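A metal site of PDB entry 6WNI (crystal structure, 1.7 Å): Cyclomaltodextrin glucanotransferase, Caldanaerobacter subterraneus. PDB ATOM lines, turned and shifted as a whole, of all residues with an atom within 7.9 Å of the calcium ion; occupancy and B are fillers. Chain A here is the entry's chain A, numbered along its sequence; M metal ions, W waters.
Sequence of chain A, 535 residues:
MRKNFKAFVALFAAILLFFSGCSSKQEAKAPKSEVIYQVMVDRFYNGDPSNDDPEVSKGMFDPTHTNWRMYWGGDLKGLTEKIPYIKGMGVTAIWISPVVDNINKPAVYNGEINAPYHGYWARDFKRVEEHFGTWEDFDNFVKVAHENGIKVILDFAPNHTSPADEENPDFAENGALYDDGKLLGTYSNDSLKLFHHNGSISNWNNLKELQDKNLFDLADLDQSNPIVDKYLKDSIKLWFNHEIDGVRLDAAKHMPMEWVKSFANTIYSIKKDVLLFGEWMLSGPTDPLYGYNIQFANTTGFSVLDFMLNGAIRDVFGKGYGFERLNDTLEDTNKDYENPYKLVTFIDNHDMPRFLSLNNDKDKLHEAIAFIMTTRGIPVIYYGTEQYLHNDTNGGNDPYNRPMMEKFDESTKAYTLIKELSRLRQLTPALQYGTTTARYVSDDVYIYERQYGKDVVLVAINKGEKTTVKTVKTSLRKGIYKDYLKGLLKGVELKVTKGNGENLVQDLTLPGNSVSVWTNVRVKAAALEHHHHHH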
ATOM      1  N   PRO A  54     -28.675 -17.869 -33.450  1.00  0.00           N
ATOM      2  CA  PRO A  54     -27.668 -17.869 -34.523  1.00  0.00           C
ATOM      3  C   PRO A  54     -27.750 -19.124 -35.383  1.00  0.00           C
ATOM      4  O   PRO A  54     -28.048 -20.217 -34.925  1.00  0.00           O
ATOM      5  CB  PRO A  54     -26.340 -17.824 -33.746  1.00  0.00           C
ATOM      6  CG  PRO A  54     -26.712 -17.298 -32.375  1.00  0.00           C
ATOM      7  CD  PRO A  54     -28.065 -17.875 -32.122  1.00  0.00           C
ATOM      8  N   VAL A  56     -25.497 -20.980 -36.637  1.00  0.00           N
ATOM      9  CA  VAL A  56     -24.580 -22.061 -36.299  1.00  0.00           C
ATOM     10  C   VAL A  56     -25.080 -22.901 -35.123  1.00  0.00           C
ATOM     11  O   VAL A  56     -24.636 -24.044 -34.941  1.00  0.00           O
ATOM     12  CB  VAL A  56     -23.182 -21.467 -36.010  1.00  0.00           C
ATOM     13  CG1 VAL A  56     -23.167 -20.748 -34.641  1.00  0.00           C
ATOM     14  CG2 VAL A  56     -22.097 -22.526 -36.096  1.00  0.00           C
ATOM     15  N   SER A  57     -26.012 -22.362 -34.338  1.00  0.00           N
ATOM     16  CA  SER A  57     -26.492 -23.005 -33.115  1.00  0.00           C
ATOM     17  C   SER A  57     -27.981 -22.759 -32.960  1.00  0.00           C
ATOM     18  O   SER A  57     -28.467 -22.413 -31.888  1.00  0.00           O
ATOM     19  CB  SER A  57     -25.742 -22.469 -31.897  1.00  0.00           C
ATOM     20  OG  SER A  57     -25.794 -21.062 -31.857  1.00  0.00           O
ATOM     21  N   MET A  60     -32.295 -23.240 -30.122  1.00  0.00           N
ATOM     22  CA  MET A  60     -32.203 -23.277 -28.671  1.00  0.00           C
ATOM     23  C   MET A  60     -32.661 -21.973 -28.032  1.00  0.00           C
ATOM     24  O   MET A  60     -32.326 -21.707 -26.879  1.00  0.00           O
ATOM     25  CB  MET A  60     -30.774 -23.582 -28.219  1.00  0.00           C
ATOM     26  CG  MET A  60     -30.261 -24.925 -28.646  1.00  0.00           C
ATOM     27  SD  MET A  60     -28.628 -25.268 -28.017  1.00  0.00           S
ATOM     28  CE  MET A  60     -27.585 -24.208 -29.005  1.00  0.00           C
ATOM     29  N   TYR A  71     -32.056 -20.665 -24.253  1.00  0.00           N
ATOM     30  CA  TYR A  71     -31.581 -19.295 -24.265  1.00  0.00           C
ATOM     31  C   TYR A  71     -32.775 -18.356 -24.345  1.00  0.00           C
ATOM     32  O   TYR A  71     -33.712 -18.594 -25.104  1.00  0.00           O
ATOM     33  CB  TYR A  71     -30.694 -19.023 -25.473  1.00  0.00           C
ATOM     34  CG  TYR A  71     -29.283 -19.557 -25.472  1.00  0.00           C
ATOM     35  CD1 TYR A  71     -28.255 -18.824 -24.889  1.00  0.00           C
ATOM     36  CD2 TYR A  71     -28.970 -20.731 -26.131  1.00  0.00           C
ATOM     37  CE1 TYR A  71     -26.935 -19.284 -24.935  1.00  0.00           C
ATOM     38  CE2 TYR A  71     -27.660 -21.205 -26.177  1.00  0.00           C
ATOM     39  CZ  TYR A  71     -26.645 -20.477 -25.589  1.00  0.00           C
ATOM     40  OH  TYR A  71     -25.351 -20.934 -25.654  1.00  0.00           O
ATOM     41  N   VAL A 100     -17.429 -18.002 -22.712  1.00  0.00           N
ATOM     42  CA  VAL A 100     -16.784 -18.841 -23.717  1.00  0.00           C
ATOM     43  C   VAL A 100     -17.851 -19.555 -24.554  1.00  0.00           C
ATOM     44  O   VAL A 100     -18.993 -19.762 -24.114  1.00  0.00           O
ATOM     45  CB  VAL A 100     -15.825 -19.884 -23.102  1.00  0.00           C
ATOM     46  CG1 VAL A 100     -14.692 -19.209 -22.362  1.00  0.00           C
ATOM     47  CG2 VAL A 100     -16.582 -20.868 -22.215  1.00  0.00           C
ATOM     48  N   ASP A 101     -17.477 -19.910 -25.789  1.00  0.00           N
ATOM     49  CA  ASP A 101     -18.371 -20.620 -26.699  1.00  0.00           C
ATOM     50  C   ASP A 101     -18.867 -21.927 -26.081  1.00  0.00           C
ATOM     51  O   ASP A 101     -18.068 -22.811 -25.751  1.00  0.00           O
ATOM     52  CB  ASP A 101     -17.613 -20.891 -28.011  1.00  0.00           C
ATOM     53  CG  ASP A 101     -18.500 -21.420 -29.139  1.00  0.00           C
ATOM     54  OD1 ASP A 101     -19.748 -21.480 -28.985  1.00  0.00           O
ATOM     55  OD2 ASP A 101     -17.944 -21.782 -30.197  1.00  0.00           O
ATOM     56  N   ASN A 102     -20.178 -22.047 -25.923  1.00  0.00           N
ATOM     57  CA  ASN A 102     -20.827 -23.244 -25.423  1.00  0.00           C
ATOM     58  C   ASN A 102     -21.412 -24.066 -26.573  1.00  0.00           C
ATOM     59  O   ASN A 102     -21.558 -23.584 -27.687  1.00  0.00           O
ATOM     60  CB  ASN A 102     -21.944 -22.875 -24.425  1.00  0.00           C
ATOM     61  CG  ASN A 102     -21.445 -22.735 -23.003  1.00  0.00           C
ATOM     62  OD1 ASN A 102     -22.127 -23.181 -22.068  1.00  0.00           O
ATOM     63  ND2 ASN A 102     -20.289 -22.129 -22.811  1.00  0.00           N
ATOM     64  N   ILE A 103     -21.761 -25.324 -26.261  1.00  0.00           N
ATOM     65  CA  ILE A 103     -22.166 -26.263 -27.310  1.00  0.00           C
ATOM     66  C   ILE A 103     -23.264 -25.683 -28.191  1.00  0.00           C
ATOM     67  O   ILE A 103     -24.172 -24.995 -27.733  1.00  0.00           O
ATOM     68  CB  ILE A 103     -22.625 -27.613 -26.705  1.00  0.00           C
ATOM     69  CG1 ILE A 103     -23.792 -27.410 -25.735  1.00  0.00           C
ATOM     70  CG2 ILE A 103     -21.452 -28.317 -26.064  1.00  0.00           C
ATOM     71  CD1 ILE A 103     -24.334 -28.741 -25.134  1.00  0.00           C
ATOM     72  N   ASN A 104     -23.179 -26.011 -29.482  1.00  0.00           N
ATOM     73  CA  ASN A 104     -24.054 -25.468 -30.514  1.00  0.00           C
ATOM     74  C   ASN A 104     -25.232 -26.366 -30.834  1.00  0.00           C
ATOM     75  O   ASN A 104     -26.042 -26.009 -31.700  1.00  0.00           O
ATOM     76  CB  ASN A 104     -23.241 -25.201 -31.785  1.00  0.00           C
ATOM     77  CG  ASN A 104     -22.243 -24.113 -31.571  1.00  0.00           C
ATOM     78  OD1 ASN A 104     -22.344 -23.361 -30.605  1.00  0.00           O
ATOM     79  ND2 ASN A 104     -21.254 -24.007 -32.481  1.00  0.00           N
ATOM     80  N   LYS A 105     -25.350 -27.500 -30.158  1.00  0.00           N
ATOM     81  CA  LYS A 105     -26.489 -28.401 -30.190  1.00  0.00           C
ATOM     82  C   LYS A 105     -26.924 -28.649 -28.760  1.00  0.00           C
ATOM     83  O   LYS A 105     -26.070 -28.719 -27.858  1.00  0.00           O
ATOM     84  CB  LYS A 105     -26.130 -29.734 -30.878  1.00  0.00           C
ATOM     85  CG  LYS A 105     -25.776 -29.563 -32.345  1.00  0.00           C
ATOM     86  CD  LYS A 105     -25.337 -30.867 -32.990  1.00  0.00           C
ATOM     87  CE  LYS A 105     -25.536 -30.810 -34.500  1.00  0.00           C
ATOM     88  NZ  LYS A 105     -25.157 -29.477 -35.058  1.00  0.00           N
ATOM     89  N   PRO A 116     -27.321 -24.647 -23.370  1.00  0.00           N
ATOM     90  CA  PRO A 116     -26.286 -24.151 -22.453  1.00  0.00           C
ATOM     91  C   PRO A 116     -26.393 -22.664 -22.169  1.00  0.00           C
ATOM     92  O   PRO A 116     -25.404 -21.928 -22.209  1.00  0.00           O
ATOM     93  CB  PRO A 116     -24.998 -24.495 -23.211  1.00  0.00           C
ATOM     94  CG  PRO A 116     -25.380 -24.209 -24.638  1.00  0.00           C
ATOM     95  CD  PRO A 116     -26.816 -24.724 -24.761  1.00  0.00           C
ATOM     96  N   TRP A 121     -21.199 -25.094 -20.164  1.00  0.00           N
ATOM     97  CA  TRP A 121     -21.019 -26.263 -21.021  1.00  0.00           C
ATOM     98  C   TRP A 121     -20.175 -25.857 -22.237  1.00  0.00           C
ATOM     99  O   TRP A 121     -20.688 -25.764 -23.362  1.00  0.00           O
ATOM    100  CB  TRP A 121     -22.350 -26.827 -21.474  1.00  0.00           C
ATOM    101  CG  TRP A 121     -23.245 -27.366 -20.375  1.00  0.00           C
ATOM    102  CD1 TRP A 121     -22.935 -27.544 -19.054  1.00  0.00           C
ATOM    103  CD2 TRP A 121     -24.584 -27.818 -20.538  1.00  0.00           C
ATOM    104  NE1 TRP A 121     -24.022 -28.064 -18.380  1.00  0.00           N
ATOM    105  CE2 TRP A 121     -25.041 -28.237 -19.274  1.00  0.00           C
ATOM    106  CE3 TRP A 121     -25.454 -27.896 -21.627  1.00  0.00           C
ATOM    107  CZ2 TRP A 121     -26.325 -28.738 -19.074  1.00  0.00           C
ATOM    108  CZ3 TRP A 121     -26.736 -28.383 -21.431  1.00  0.00           C
ATOM    109  CH2 TRP A 121     -27.150 -28.814 -20.171  1.00  0.00           C
ATOM    110  N   ARG A 123     -17.670 -25.502 -25.374  1.00  0.00           N
ATOM    111  CA  ARG A 123     -17.091 -26.210 -26.505  1.00  0.00           C
ATOM    112  C   ARG A 123     -15.752 -25.624 -26.961  1.00  0.00           C
ATOM    113  O   ARG A 123     -14.973 -26.339 -27.597  1.00  0.00           O
ATOM    114  CB  ARG A 123     -18.075 -26.249 -27.693  1.00  0.00           C
ATOM    115  CG  ARG A 123     -18.014 -25.039 -28.608  1.00  0.00           C
ATOM    116  CD  ARG A 123     -19.178 -24.970 -29.564  1.00  0.00           C
ATOM    117  NE  ARG A 123     -19.338 -26.082 -30.513  1.00  0.00           N
ATOM    118  CZ  ARG A 123     -18.770 -26.148 -31.721  1.00  0.00           C
ATOM    119  NH1 ARG A 123     -17.930 -25.214 -32.141  1.00  0.00           N
ATOM    120  NH2 ARG A 123     -19.042 -27.184 -32.505  1.00  0.00           N
ATOM    121  N   ASP A 124     -15.446 -24.365 -26.601  1.00  0.00           N
ATOM    122  CA  ASP A 124     -14.251 -23.702 -27.108  1.00  0.00           C
ATOM    123  C   ASP A 124     -13.881 -22.574 -26.154  1.00  0.00           C
ATOM    124  O   ASP A 124     -14.566 -21.543 -26.121  1.00  0.00           O
ATOM    125  CB  ASP A 124     -14.529 -23.176 -28.518  1.00  0.00           C
ATOM    126  CG  ASP A 124     -13.265 -22.777 -29.263  1.00  0.00           C
ATOM    127  OD1 ASP A 124     -12.258 -22.431 -28.623  1.00  0.00           O
ATOM    128  OD2 ASP A 124     -13.310 -22.789 -30.510  1.00  0.00           O
ATOM    129  N   VAL A 128     -15.723 -16.448 -28.134  1.00  0.00           N
ATOM    130  CA  VAL A 128     -16.895 -15.906 -27.451  1.00  0.00           C
ATOM    131  C   VAL A 128     -18.130 -16.659 -27.922  1.00  0.00           C
ATOM    132  O   VAL A 128     -18.263 -17.021 -29.100  1.00  0.00           O
ATOM    133  CB  VAL A 128     -17.017 -14.386 -27.706  1.00  0.00           C
ATOM    134  CG1 VAL A 128     -18.212 -13.830 -26.926  1.00  0.00           C
ATOM    135  CG2 VAL A 128     -15.747 -13.683 -27.301  1.00  0.00           C
ATOM    136  N   GLU A 129     -19.029 -16.934 -26.984  1.00  0.00           N
ATOM    137  CA  GLU A 129     -20.329 -17.523 -27.310  1.00  0.00           C
ATOM    138  C   GLU A 129     -21.099 -16.607 -28.248  1.00  0.00           C
ATOM    139  O   GLU A 129     -21.371 -15.449 -27.920  1.00  0.00           O
ATOM    140  CB  GLU A 129     -21.122 -17.732 -26.011  1.00  0.00           C
ATOM    141  CG  GLU A 129     -22.564 -18.132 -26.249  1.00  0.00           C
ATOM    142  CD  GLU A 129     -22.677 -19.287 -27.207  1.00  0.00           C
ATOM    143  OE1 GLU A 129     -21.972 -20.301 -26.995  1.00  0.00           O
ATOM    144  OE2 GLU A 129     -23.448 -19.176 -28.202  1.00  0.00           O
ATOM    145  N   GLU A 130     -21.486 -17.153 -29.412  1.00  0.00           N
ATOM    146  CA  GLU A 130     -22.113 -16.341 -30.447  1.00  0.00           C
ATOM    147  C   GLU A 130     -23.509 -15.853 -30.061  1.00  0.00           C
ATOM    148  O   GLU A 130     -23.987 -14.865 -30.622  1.00  0.00           O
ATOM    149  CB  GLU A 130     -22.151 -17.120 -31.775  1.00  0.00           C
ATOM    150  CG  GLU A 130     -23.091 -18.317 -31.840  1.00  0.00           C
ATOM    151  CD  GLU A 130     -22.632 -19.532 -31.022  1.00  0.00           C
ATOM    152  OE1 GLU A 130     -21.462 -19.563 -30.605  1.00  0.00           O
ATOM    153  OE2 GLU A 130     -23.425 -20.467 -30.827  1.00  0.00           O
ATOM    154  N   HIS A 131     -24.182 -16.514 -29.104  1.00  0.00           N
ATOM    155  CA  HIS A 131     -25.477 -15.966 -28.615  1.00  0.00           C
ATOM    156  C   HIS A 131     -25.264 -14.650 -27.867  1.00  0.00           C
ATOM    157  O   HIS A 131     -26.171 -13.884 -27.784  1.00  0.00           O
ATOM    158  CB  HIS A 131     -26.184 -16.972 -27.687  1.00  0.00           C
ATOM    159  CG  HIS A 131     -26.755 -18.155 -28.392  1.00  0.00           C
ATOM    160  ND1 HIS A 131     -26.007 -19.207 -28.849  1.00  0.00           N
ATOM    161  CD2 HIS A 131     -28.016 -18.456 -28.730  1.00  0.00           C
ATOM    162  CE1 HIS A 131     -26.779 -20.074 -29.425  1.00  0.00           C
ATOM    163  NE2 HIS A 131     -28.010 -19.657 -29.326  1.00  0.00           N
ATOM    164  N   PHE A 132     -24.075 -14.429 -27.311  1.00  0.00           N
ATOM    165  CA  PHE A 132     -23.800 -13.265 -26.486  1.00  0.00           C
ATOM    166  C   PHE A 132     -23.054 -12.187 -27.227  1.00  0.00           C
ATOM    167  O   PHE A 132     -23.126 -11.009 -26.835  1.00  0.00           O
ATOM    168  CB  PHE A 132     -22.982 -13.654 -25.240  1.00  0.00           C
ATOM    169  CG  PHE A 132     -23.650 -14.698 -24.358  1.00  0.00           C
ATOM    170  CD1 PHE A 132     -25.027 -14.891 -24.372  1.00  0.00           C
ATOM    171  CD2 PHE A 132     -22.872 -15.494 -23.516  1.00  0.00           C
ATOM    172  CE1 PHE A 132     -25.628 -15.858 -23.568  1.00  0.00           C
ATOM    173  CE2 PHE A 132     -23.471 -16.462 -22.688  1.00  0.00           C
ATOM    174  CZ  PHE A 132     -24.851 -16.646 -22.722  1.00  0.00           C
ATOM    175  N   GLU A 173     -23.111 -32.412 -27.982  1.00  0.00           N
ATOM    176  CA  GLU A 173     -21.941 -32.412 -28.856  1.00  0.00           C
ATOM    177  C   GLU A 173     -20.872 -33.376 -28.352  1.00  0.00           C
ATOM    178  O   GLU A 173     -19.688 -33.194 -28.637  1.00  0.00           O
ATOM    179  CB  GLU A 173     -21.393 -30.994 -29.022  1.00  0.00           C
ATOM    180  CG  GLU A 173     -22.261 -30.097 -29.919  1.00  0.00           C
ATOM    181  CD  GLU A 173     -21.538 -28.886 -30.481  1.00  0.00           C
ATOM    182  OE1 GLU A 173     -21.100 -28.019 -29.703  1.00  0.00           O
ATOM    183  OE2 GLU A 173     -21.397 -28.770 -31.725  1.00  0.00           O
HETATM  184 CA    CA M   1     -22.131 -21.614 -29.092  1.00  0.00          CA
HETATM  185  O   HOH W   1     -24.314 -22.173 -28.154  1.00  0.00           O
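The guanidinium group of Arg 123 lies close to the side-chain amide nitrogen of Asn 104 (3.4 Å).
The side-chain carboxylate (OE1) of Glu 173 sits at hydrogen-bond distance from the backbone NH (N) of Asn 104.
OD2 of Asp 101 lies within salt-bridge range of NH1 of Arg 123 (3.9 Å).
O of Asp 101 is in hydrogen-bond range of N of Asp 124 (3.2 Å).
The side-chain carboxylate (OE2) of Glu 130 lies close to the side-chain hydroxyl (OG) of Ser 57.
ND1 of His 131 lies within hydrogen-bond range of OE2 of Glu 129.
ND2 of Asn 102 lies within hydrogen-bond range of O of Val 100, at 3.0 Å.
The backbone NH (N) of Trp 121 sits at hydrogen-bond distance from the side-chain amide oxygen (OD1) of Asn 102 (2.9 Å).
Water W1 lies within hydrogen-bond range of O of Ile 103, OH of Tyr 71, OE2 of Glu 129 and ND1 of His 131.
The calcium ion is bound by OD1 of Asn 104 (2.3 Å), OD1 of Asp 101 (2.4 Å), water W1 (2.4 Å), OE2 of Glu 130 (2.4 Å), OE1 of Glu 129 (2.5 Å), O of Asn 102 (2.5 Å) and OE1 of Glu 130 (2.6 Å).
Slightly farther from the calcium ion lies OE2 of Glu 129 (2.9 Å).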
